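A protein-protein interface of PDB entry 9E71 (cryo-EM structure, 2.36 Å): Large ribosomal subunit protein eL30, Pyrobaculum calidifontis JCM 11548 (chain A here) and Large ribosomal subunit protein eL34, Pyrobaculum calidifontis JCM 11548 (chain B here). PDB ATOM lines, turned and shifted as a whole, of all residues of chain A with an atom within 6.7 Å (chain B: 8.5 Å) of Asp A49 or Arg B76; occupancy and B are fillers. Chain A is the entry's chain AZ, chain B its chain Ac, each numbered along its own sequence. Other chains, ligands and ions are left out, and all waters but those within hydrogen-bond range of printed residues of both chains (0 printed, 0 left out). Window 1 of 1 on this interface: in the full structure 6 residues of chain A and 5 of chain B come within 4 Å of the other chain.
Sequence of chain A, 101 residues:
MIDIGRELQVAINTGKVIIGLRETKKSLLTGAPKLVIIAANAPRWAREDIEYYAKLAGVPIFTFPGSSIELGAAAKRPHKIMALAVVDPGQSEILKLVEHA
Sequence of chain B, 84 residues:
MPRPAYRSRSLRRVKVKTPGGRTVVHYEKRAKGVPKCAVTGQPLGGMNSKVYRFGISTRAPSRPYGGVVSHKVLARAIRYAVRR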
ATOM      1  N   LEU A  21     -11.308  17.337  15.000  1.00  0.00           N
ATOM      2  CA  LEU A  21     -10.444  16.987  13.878  1.00  0.00           C
ATOM      3  C   LEU A  21     -10.734  17.851  12.658  1.00  0.00           C
ATOM      4  O   LEU A  21      -9.808  18.294  11.973  1.00  0.00           O
ATOM      5  CB  LEU A  21     -10.601  15.505  13.541  1.00  0.00           C
ATOM      6  CG  LEU A  21      -9.562  14.883  12.609  1.00  0.00           C
ATOM      7  CD1 LEU A  21     -10.039  14.926  11.169  1.00  0.00           C
ATOM      8  CD2 LEU A  21      -8.229  15.587  12.750  1.00  0.00           C
ATOM      9  N   LYS A  25      -8.147  20.473  11.034  1.00  0.00           N
ATOM     10  CA  LYS A  25      -7.735  20.382   9.638  1.00  0.00           C
ATOM     11  C   LYS A  25      -7.935  21.706   8.914  1.00  0.00           C
ATOM     12  O   LYS A  25      -7.072  22.139   8.144  1.00  0.00           O
ATOM     13  CB  LYS A  25      -8.498  19.242   8.954  1.00  0.00           C
ATOM     14  CG  LYS A  25      -8.818  19.401   7.464  1.00  0.00           C
ATOM     15  CD  LYS A  25     -10.166  20.084   7.198  1.00  0.00           C
ATOM     16  CE  LYS A  25     -11.326  19.287   7.753  1.00  0.00           C
ATOM     17  NZ  LYS A  25     -12.540  20.139   7.851  1.00  0.00           N
ATOM     18  N   LEU A  28      -5.356  24.187  10.078  1.00  0.00           N
ATOM     19  CA  LEU A  28      -4.063  23.878   9.492  1.00  0.00           C
ATOM     20  C   LEU A  28      -4.010  24.300   8.028  1.00  0.00           C
ATOM     21  O   LEU A  28      -2.976  24.776   7.548  1.00  0.00           O
ATOM     22  CB  LEU A  28      -3.790  22.387   9.630  1.00  0.00           C
ATOM     23  CG  LEU A  28      -2.345  22.007   9.917  1.00  0.00           C
ATOM     24  CD1 LEU A  28      -2.260  20.549  10.353  1.00  0.00           C
ATOM     25  CD2 LEU A  28      -1.446  22.303   8.749  1.00  0.00           C
ATOM     26  N   ARG A  44      -5.644   5.677  11.287  1.00  0.00           N
ATOM     27  CA  ARG A  44      -4.542   5.773  10.338  1.00  0.00           C
ATOM     28  C   ARG A  44      -4.766   6.907   9.340  1.00  0.00           C
ATOM     29  O   ARG A  44      -3.856   7.704   9.069  1.00  0.00           O
ATOM     30  CB  ARG A  44      -4.393   4.404   9.660  1.00  0.00           C
ATOM     31  CG  ARG A  44      -3.327   4.225   8.604  1.00  0.00           C
ATOM     32  CD  ARG A  44      -3.807   4.602   7.209  1.00  0.00           C
ATOM     33  NE  ARG A  44      -3.105   3.848   6.177  1.00  0.00           N
ATOM     34  CZ  ARG A  44      -3.272   2.553   5.949  1.00  0.00           C
ATOM     35  NH1 ARG A  44      -4.134   1.833   6.647  1.00  0.00           N
ATOM     36  NH2 ARG A  44      -2.565   1.969   4.986  1.00  0.00           N
ATOM     37  N   TRP A  45      -5.990   7.019   8.814  1.00  0.00           N
ATOM     38  CA  TRP A  45      -6.291   8.058   7.833  1.00  0.00           C
ATOM     39  C   TRP A  45      -6.196   9.452   8.445  1.00  0.00           C
ATOM     40  O   TRP A  45      -5.632  10.366   7.836  1.00  0.00           O
ATOM     41  CB  TRP A  45      -7.674   7.813   7.216  1.00  0.00           C
ATOM     42  CG  TRP A  45      -8.809   7.747   8.199  1.00  0.00           C
ATOM     43  CD1 TRP A  45      -9.270   6.641   8.846  1.00  0.00           C
ATOM     44  CD2 TRP A  45      -9.622   8.837   8.640  1.00  0.00           C
ATOM     45  NE1 TRP A  45     -10.317   6.975   9.668  1.00  0.00           N
ATOM     46  CE2 TRP A  45     -10.550   8.321   9.561  1.00  0.00           C
ATOM     47  CE3 TRP A  45      -9.643  10.205   8.358  1.00  0.00           C
ATOM     48  CZ2 TRP A  45     -11.498   9.120  10.190  1.00  0.00           C
ATOM     49  CZ3 TRP A  45     -10.583  10.994   8.981  1.00  0.00           C
ATOM     50  CH2 TRP A  45     -11.497  10.452   9.885  1.00  0.00           C
ATOM     51  N   ALA A  46      -6.713   9.628   9.661  1.00  0.00           N
ATOM     52  CA  ALA A  46      -6.678  10.941  10.292  1.00  0.00           C
ATOM     53  C   ALA A  46      -5.259  11.315  10.691  1.00  0.00           C
ATOM     54  O   ALA A  46      -4.852  12.477  10.562  1.00  0.00           O
ATOM     55  CB  ALA A  46      -7.605  10.961  11.504  1.00  0.00           C
ATOM     56  N   ARG A  47      -4.490  10.334  11.163  1.00  0.00           N
ATOM     57  CA  ARG A  47      -3.102  10.568  11.535  1.00  0.00           C
ATOM     58  C   ARG A  47      -2.280  11.011  10.330  1.00  0.00           C
ATOM     59  O   ARG A  47      -1.532  11.993  10.403  1.00  0.00           O
ATOM     60  CB  ARG A  47      -2.537   9.297  12.167  1.00  0.00           C
ATOM     61  CG  ARG A  47      -1.075   9.038  11.930  1.00  0.00           C
ATOM     62  CD  ARG A  47      -0.444   8.361  13.137  1.00  0.00           C
ATOM     63  NE  ARG A  47      -1.246   7.248  13.634  1.00  0.00           N
ATOM     64  CZ  ARG A  47      -1.897   7.248  14.791  1.00  0.00           C
ATOM     65  NH1 ARG A  47      -1.853   8.287  15.609  1.00  0.00           N
ATOM     66  NH2 ARG A  47      -2.607   6.180  15.137  1.00  0.00           N
ATOM     67  N   GLU A  48      -2.446  10.334   9.188  1.00  0.00           N
ATOM     68  CA  GLU A  48      -1.699  10.751   8.004  1.00  0.00           C
ATOM     69  C   GLU A  48      -2.209  12.060   7.418  1.00  0.00           C
ATOM     70  O   GLU A  48      -1.418  12.829   6.862  1.00  0.00           O
ATOM     71  CB  GLU A  48      -1.688   9.661   6.940  1.00  0.00           C
ATOM     72  CG  GLU A  48      -0.707   8.567   7.263  1.00  0.00           C
ATOM     73  CD  GLU A  48      -1.183   7.205   6.885  1.00  0.00           C
ATOM     74  OE1 GLU A  48      -1.487   6.427   7.798  1.00  0.00           O
ATOM     75  OE2 GLU A  48      -1.220   6.905   5.674  1.00  0.00           O
ATOM     76  N   ASP A  49      -3.511  12.338   7.524  1.00  0.00           N
ATOM     77  CA  ASP A  49      -4.017  13.627   7.059  1.00  0.00           C
ATOM     78  C   ASP A  49      -3.407  14.770   7.858  1.00  0.00           C
ATOM     79  O   ASP A  49      -2.923  15.758   7.287  1.00  0.00           O
ATOM     80  CB  ASP A  49      -5.540  13.665   7.161  1.00  0.00           C
ATOM     81  CG  ASP A  49      -6.224  13.159   5.909  1.00  0.00           C
ATOM     82  OD1 ASP A  49      -5.669  12.261   5.246  1.00  0.00           O
ATOM     83  OD2 ASP A  49      -7.313  13.668   5.576  1.00  0.00           O
ATOM     84  N   ILE A  50      -3.392  14.632   9.184  1.00  0.00           N
ATOM     85  CA  ILE A  50      -2.836  15.680  10.029  1.00  0.00           C
ATOM     86  C   ILE A  50      -1.337  15.815   9.806  1.00  0.00           C
ATOM     87  O   ILE A  50      -0.815  16.931   9.732  1.00  0.00           O
ATOM     88  CB  ILE A  50      -3.170  15.420  11.504  1.00  0.00           C
ATOM     89  CG1 ILE A  50      -4.669  15.582  11.741  1.00  0.00           C
ATOM     90  CG2 ILE A  50      -2.398  16.372  12.385  1.00  0.00           C
ATOM     91  CD1 ILE A  50      -5.166  16.977  11.497  1.00  0.00           C
ATOM     92  N   GLU A  51      -0.621  14.691   9.681  1.00  0.00           N
ATOM     93  CA  GLU A  51       0.820  14.757   9.453  1.00  0.00           C
ATOM     94  C   GLU A  51       1.153  15.411   8.117  1.00  0.00           C
ATOM     95  O   GLU A  51       2.055  16.252   8.041  1.00  0.00           O
ATOM     96  CB  GLU A  51       1.443  13.366   9.548  1.00  0.00           C
ATOM     97  CG  GLU A  51       1.874  13.008  10.955  1.00  0.00           C
ATOM     98  CD  GLU A  51       1.713  11.542  11.286  1.00  0.00           C
ATOM     99  OE1 GLU A  51       0.941  11.230  12.212  1.00  0.00           O
ATOM    100  OE2 GLU A  51       2.374  10.705  10.638  1.00  0.00           O
ATOM    101  N   TYR A  52       0.422  15.059   7.056  1.00  0.00           N
ATOM    102  CA  TYR A  52       0.684  15.643   5.744  1.00  0.00           C
ATOM    103  C   TYR A  52       0.400  17.140   5.734  1.00  0.00           C
ATOM    104  O   TYR A  52       1.210  17.937   5.237  1.00  0.00           O
ATOM    105  CB  TYR A  52      -0.156  14.933   4.688  1.00  0.00           C
ATOM    106  CG  TYR A  52       0.040  15.465   3.290  1.00  0.00           C
ATOM    107  CD1 TYR A  52       1.241  15.292   2.620  1.00  0.00           C
ATOM    108  CD2 TYR A  52      -0.976  16.152   2.643  1.00  0.00           C
ATOM    109  CE1 TYR A  52       1.420  15.782   1.345  1.00  0.00           C
ATOM    110  CE2 TYR A  52      -0.807  16.644   1.375  1.00  0.00           C
ATOM    111  CZ  TYR A  52       0.392  16.456   0.728  1.00  0.00           C
ATOM    112  OH  TYR A  52       0.559  16.946  -0.543  1.00  0.00           O
ATOM    113  N   TYR A  53      -0.742  17.544   6.298  1.00  0.00           N
ATOM    114  CA  TYR A  53      -1.080  18.963   6.301  1.00  0.00           C
ATOM    115  C   TYR A  53      -0.117  19.760   7.170  1.00  0.00           C
ATOM    116  O   TYR A  53       0.310  20.853   6.782  1.00  0.00           O
ATOM    117  CB  TYR A  53      -2.518  19.160   6.772  1.00  0.00           C
ATOM    118  CG  TYR A  53      -3.534  18.649   5.786  1.00  0.00           C
ATOM    119  CD1 TYR A  53      -3.234  18.579   4.436  1.00  0.00           C
ATOM    120  CD2 TYR A  53      -4.786  18.220   6.202  1.00  0.00           C
ATOM    121  CE1 TYR A  53      -4.148  18.107   3.527  1.00  0.00           C
ATOM    122  CE2 TYR A  53      -5.709  17.743   5.298  1.00  0.00           C
ATOM    123  CZ  TYR A  53      -5.383  17.691   3.959  1.00  0.00           C
ATOM    124  OH  TYR A  53      -6.295  17.220   3.045  1.00  0.00           O
ATOM    125  N   ALA A  54       0.247  19.232   8.340  1.00  0.00           N
ATOM    126  CA  ALA A  54       1.149  19.960   9.221  1.00  0.00           C
ATOM    127  C   ALA A  54       2.544  20.049   8.625  1.00  0.00           C
ATOM    128  O   ALA A  54       3.234  21.057   8.802  1.00  0.00           O
ATOM    129  CB  ALA A  54       1.191  19.299  10.598  1.00  0.00           C
ATOM    130  N   SER B  70     -18.066   4.751  -4.080  1.00  0.00           N
ATOM    131  CA  SER B  70     -18.731   5.955  -3.622  1.00  0.00           C
ATOM    132  C   SER B  70     -17.766   7.138  -3.615  1.00  0.00           C
ATOM    133  O   SER B  70     -16.549   6.998  -3.798  1.00  0.00           O
ATOM    134  CB  SER B  70     -19.318   5.741  -2.229  1.00  0.00           C
ATOM    135  OG  SER B  70     -18.351   5.194  -1.357  1.00  0.00           O
ATOM    136  N   HIS B  71     -18.337   8.322  -3.390  1.00  0.00           N
ATOM    137  CA  HIS B  71     -17.540   9.542  -3.378  1.00  0.00           C
ATOM    138  C   HIS B  71     -16.542   9.541  -2.225  1.00  0.00           C
ATOM    139  O   HIS B  71     -15.437  10.073  -2.362  1.00  0.00           O
ATOM    140  CB  HIS B  71     -18.455  10.767  -3.321  1.00  0.00           C
ATOM    141  CG  HIS B  71     -19.160  10.942  -2.012  1.00  0.00           C
ATOM    142  ND1 HIS B  71     -20.285  10.226  -1.671  1.00  0.00           N
ATOM    143  CD2 HIS B  71     -18.885  11.739  -0.953  1.00  0.00           C
ATOM    144  CE1 HIS B  71     -20.679  10.580  -0.461  1.00  0.00           C
ATOM    145  NE2 HIS B  71     -19.849  11.499  -0.005  1.00  0.00           N
ATOM    146  N   LYS B  72     -16.898   8.921  -1.095  1.00  0.00           N
ATOM    147  CA  LYS B  72     -15.998   8.874   0.055  1.00  0.00           C
ATOM    148  C   LYS B  72     -14.743   8.077  -0.265  1.00  0.00           C
ATOM    149  O   LYS B  72     -13.615   8.544  -0.047  1.00  0.00           O
ATOM    150  CB  LYS B  72     -16.716   8.256   1.256  1.00  0.00           C
ATOM    151  CG  LYS B  72     -17.220   9.239   2.284  1.00  0.00           C
ATOM    152  CD  LYS B  72     -18.422   8.668   3.008  1.00  0.00           C
ATOM    153  CE  LYS B  72     -19.073   9.699   3.904  1.00  0.00           C
ATOM    154  NZ  LYS B  72     -18.064  10.539   4.595  1.00  0.00           N
ATOM    155  N   VAL B  73     -14.930   6.867  -0.793  1.00  0.00           N
ATOM    156  CA  VAL B  73     -13.808   6.008  -1.147  1.00  0.00           C
ATOM    157  C   VAL B  73     -12.978   6.647  -2.246  1.00  0.00           C
ATOM    158  O   VAL B  73     -11.743   6.610  -2.204  1.00  0.00           O
ATOM    159  CB  VAL B  73     -14.311   4.613  -1.557  1.00  0.00           C
ATOM    160  CG1 VAL B  73     -13.169   3.787  -2.108  1.00  0.00           C
ATOM    161  CG2 VAL B  73     -14.968   3.916  -0.379  1.00  0.00           C
ATOM    162  N   LEU B  74     -13.638   7.253  -3.237  1.00  0.00           N
ATOM    163  CA  LEU B  74     -12.906   7.876  -4.336  1.00  0.00           C
ATOM    164  C   LEU B  74     -12.062   9.049  -3.852  1.00  0.00           C
ATOM    165  O   LEU B  74     -10.892   9.175  -4.224  1.00  0.00           O
ATOM    166  CB  LEU B  74     -13.872   8.332  -5.424  1.00  0.00           C
ATOM    167  CG  LEU B  74     -13.191   9.034  -6.596  1.00  0.00           C
ATOM    168  CD1 LEU B  74     -12.380   8.048  -7.411  1.00  0.00           C
ATOM    169  CD2 LEU B  74     -14.214   9.726  -7.457  1.00  0.00           C
ATOM    170  N   ALA B  75     -12.633   9.904  -3.001  1.00  0.00           N
ATOM    171  CA  ALA B  75     -11.904  11.063  -2.501  1.00  0.00           C
ATOM    172  C   ALA B  75     -10.727  10.643  -1.632  1.00  0.00           C
ATOM    173  O   ALA B  75      -9.623  11.190  -1.759  1.00  0.00           O
ATOM    174  CB  ALA B  75     -12.849  11.972  -1.722  1.00  0.00           C
ATOM    175  N   ARG B  76     -10.937   9.663  -0.748  1.00  0.00           N
ATOM    176  CA  ARG B  76      -9.853   9.221   0.122  1.00  0.00           C
ATOM    177  C   ARG B  76      -8.742   8.548  -0.676  1.00  0.00           C
ATOM    178  O   ARG B  76      -7.552   8.772  -0.412  1.00  0.00           O
ATOM    179  CB  ARG B  76     -10.399   8.289   1.201  1.00  0.00           C
ATOM    180  CG  ARG B  76      -9.363   7.387   1.824  1.00  0.00           C
ATOM    181  CD  ARG B  76      -8.529   8.113   2.856  1.00  0.00           C
ATOM    182  NE  ARG B  76      -9.295   9.121   3.576  1.00  0.00           N
ATOM    183  CZ  ARG B  76      -8.758  10.155   4.209  1.00  0.00           C
ATOM    184  NH1 ARG B  76      -7.451  10.351   4.226  1.00  0.00           N
ATOM    185  NH2 ARG B  76      -9.553  11.017   4.834  1.00  0.00           N
ATOM    186  N   ALA B  77      -9.107   7.736  -1.673  1.00  0.00           N
ATOM    187  CA  ALA B  77      -8.100   7.109  -2.520  1.00  0.00           C
ATOM    188  C   ALA B  77      -7.334   8.147  -3.321  1.00  0.00           C
ATOM    189  O   ALA B  77      -6.119   8.017  -3.513  1.00  0.00           O
ATOM    190  CB  ALA B  77      -8.758   6.095  -3.454  1.00  0.00           C
ATOM    191  N   ILE B  78      -8.024   9.186  -3.793  1.00  0.00           N
ATOM    192  CA  ILE B  78      -7.361  10.242  -4.550  1.00  0.00           C
ATOM    193  C   ILE B  78      -6.380  10.996  -3.669  1.00  0.00           C
ATOM    194  O   ILE B  78      -5.284  11.351  -4.109  1.00  0.00           O
ATOM    195  CB  ILE B  78      -8.400  11.187  -5.174  1.00  0.00           C
ATOM    196  CG1 ILE B  78      -9.062  10.525  -6.378  1.00  0.00           C
ATOM    197  CG2 ILE B  78      -7.749  12.492  -5.574  1.00  0.00           C
ATOM    198  CD1 ILE B  78     -10.201  11.323  -6.949  1.00  0.00           C
ATOM    199  N   ARG B  79      -6.760  11.259  -2.417  1.00  0.00           N
ATOM    200  CA  ARG B  79      -5.849  11.918  -1.484  1.00  0.00           C
ATOM    201  C   ARG B  79      -4.612  11.069  -1.222  1.00  0.00           C
ATOM    202  O   ARG B  79      -3.482  11.581  -1.198  1.00  0.00           O
ATOM    203  CB  ARG B  79      -6.572  12.217  -0.174  1.00  0.00           C
ATOM    204  CG  ARG B  79      -7.462  13.433  -0.215  1.00  0.00           C
ATOM    205  CD  ARG B  79      -8.068  13.701   1.144  1.00  0.00           C
ATOM    206  NE  ARG B  79      -9.388  14.306   1.042  1.00  0.00           N
ATOM    207  CZ  ARG B  79      -9.610  15.612   1.048  1.00  0.00           C
ATOM    208  NH1 ARG B  79      -8.618  16.480   1.147  1.00  0.00           N
ATOM    209  NH2 ARG B  79     -10.859  16.056   0.958  1.00  0.00           N
ATOM    210  N   TYR B  80      -4.810   9.763  -1.018  1.00  0.00           N
ATOM    211  CA  TYR B  80      -3.682   8.867  -0.780  1.00  0.00           C
ATOM    212  C   TYR B  80      -2.755   8.821  -1.988  1.00  0.00           C
ATOM    213  O   TYR B  80      -1.528   8.856  -1.846  1.00  0.00           O
ATOM    214  CB  TYR B  80      -4.180   7.462  -0.445  1.00  0.00           C
ATOM    215  CG  TYR B  80      -4.597   7.266   0.989  1.00  0.00           C
ATOM    216  CD1 TYR B  80      -4.343   8.231   1.949  1.00  0.00           C
ATOM    217  CD2 TYR B  80      -5.249   6.108   1.383  1.00  0.00           C
ATOM    218  CE1 TYR B  80      -4.727   8.048   3.263  1.00  0.00           C
ATOM    219  CE2 TYR B  80      -5.635   5.916   2.689  1.00  0.00           C
ATOM    220  CZ  TYR B  80      -5.374   6.886   3.624  1.00  0.00           C
ATOM    221  OH  TYR B  80      -5.763   6.687   4.926  1.00  0.00           O
ATOM    222  N   ALA B  81      -3.325   8.754  -3.190  1.00  0.00           N
ATOM    223  CA  ALA B  81      -2.498   8.712  -4.389  1.00  0.00           C
ATOM    224  C   ALA B  81      -1.778  10.035  -4.608  1.00  0.00           C
ATOM    225  O   ALA B  81      -0.641  10.058  -5.096  1.00  0.00           O
ATOM    226  CB  ALA B  81      -3.353   8.354  -5.603  1.00  0.00           C
ATOM    227  N   VAL B  82      -2.427  11.150  -4.266  1.00  0.00           N
ATOM    228  CA  VAL B  82      -1.811  12.463  -4.436  1.00  0.00           C
ATOM    229  C   VAL B  82      -0.607  12.604  -3.520  1.00  0.00           C
ATOM    230  O   VAL B  82       0.446  13.110  -3.924  1.00  0.00           O
ATOM    231  CB  VAL B  82      -2.843  13.575  -4.183  1.00  0.00           C
ATOM    232  CG1 VAL B  82      -2.172  14.782  -3.560  1.00  0.00           C
ATOM    233  CG2 VAL B  82      -3.522  13.957  -5.481  1.00  0.00           C
ATOM    234  N   ARG B  83      -0.745  12.167  -2.269  1.00  0.00           N
ATOM    235  CA  ARG B  83       0.406  12.209  -1.373  1.00  0.00           C
ATOM    236  C   ARG B  83       1.471  11.205  -1.790  1.00  0.00           C
ATOM    237  O   ARG B  83       2.669  11.458  -1.626  1.00  0.00           O
ATOM    238  CB  ARG B  83      -0.030  11.958   0.066  1.00  0.00           C
ATOM    239  CG  ARG B  83      -0.997  12.990   0.571  1.00  0.00           C
ATOM    240  CD  ARG B  83      -1.556  12.620   1.916  1.00  0.00           C
ATOM    241  NE  ARG B  83      -2.867  13.221   2.103  1.00  0.00           N
ATOM    242  CZ  ARG B  83      -3.758  12.809   2.988  1.00  0.00           C
ATOM    243  NH1 ARG B  83      -3.505  11.801   3.807  1.00  0.00           N
ATOM    244  NH2 ARG B  83      -4.930  13.430   3.063  1.00  0.00           N
ATOM    245  N   ARG B  84       1.059  10.069  -2.339  1.00  0.00           N
ATOM    246  CA  ARG B  84       1.968   8.959  -2.575  1.00  0.00           C
ATOM    247  C   ARG B  84       2.587   8.998  -3.960  1.00  0.00           C
ATOM    248  O   ARG B  84       3.764   8.682  -4.123  1.00  0.00           O
ATOM    249  CB  ARG B  84       1.224   7.644  -2.366  1.00  0.00           C
ATOM    250  CG  ARG B  84       2.089   6.484  -1.936  1.00  0.00           C
ATOM    251  CD  ARG B  84       1.263   5.467  -1.161  1.00  0.00           C
ATOM    252  NE  ARG B  84       1.064   5.887   0.221  1.00  0.00           N
ATOM    253  CZ  ARG B  84       0.032   6.596   0.659  1.00  0.00           C
ATOM    254  NH1 ARG B  84      -0.939   6.978  -0.152  1.00  0.00           N
ATOM    255  NH2 ARG B  84      -0.031   6.923   1.947  1.00  0.00           N
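Arg A44 touches Tyr B80.
Arg B76 touches Trp A45 (NH2 to CE3, 3.6 Å).
OH of Tyr B80 touches CB of Trp A45 (3.2 Å).
NH1 of Arg B83 touches O of Glu A48, 3.8 Å away.
CD2 of Tyr A52 touches NE of Arg B83, 3.5 Å away.
Hydrophobic or aromatic side chains of chain B that line the printed part of chain A: Tyr B80.
Hydrophobic or aromatic side chains of chain A within 4 Å of the printed part of chain B: Trp A45, Tyr A52 and Tyr A53.
Among the printed residues, 9 pairs touch across the chains.
Among the printed residues, Asp or Glu carboxylates within 4 Å of a Lys or Arg side-chain nitrogen of the other chain: Glu A48 with Arg B84 (3.9 Å), Asp A49 with Arg B76 (2.8 Å) and Asp A49 with Arg B83 (2.6 Å).
The side-chain carboxylate (OE2) of Glu A48 lies within salt-bridge range of the guanidinium group (NH2) of Arg B84 (3.9 Å).
NH1 of Arg B76 is in salt-bridge range of OD1 of Asp A49, at 2.8 Å.
OD1 of Asp A49 is in salt-bridge range of NH2 of Arg B83 (2.6 Å).
The side-chain hydroxyl (OH) of Tyr A53 is in hydrogen-bond range of the guanidinium group (NH1) of Arg B79, at 3.1 Å.
NE of Arg A44 lies within salt-bridge range of OE1 of Glu A48, at 3.4 Å.
NH1 of Arg B84 is in hydrogen-bond range of O of Tyr B80 (2.6 Å).
Of the printed residues of chain B, Glu A48 touches Arg B83 and Arg B84.
Of the printed residues of chain B, Tyr A53 touches Arg B79 (3.1 Å).
The nearest printed residue of chain B that does not touch Trp A45 is Arg B83 (4.8 Å).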
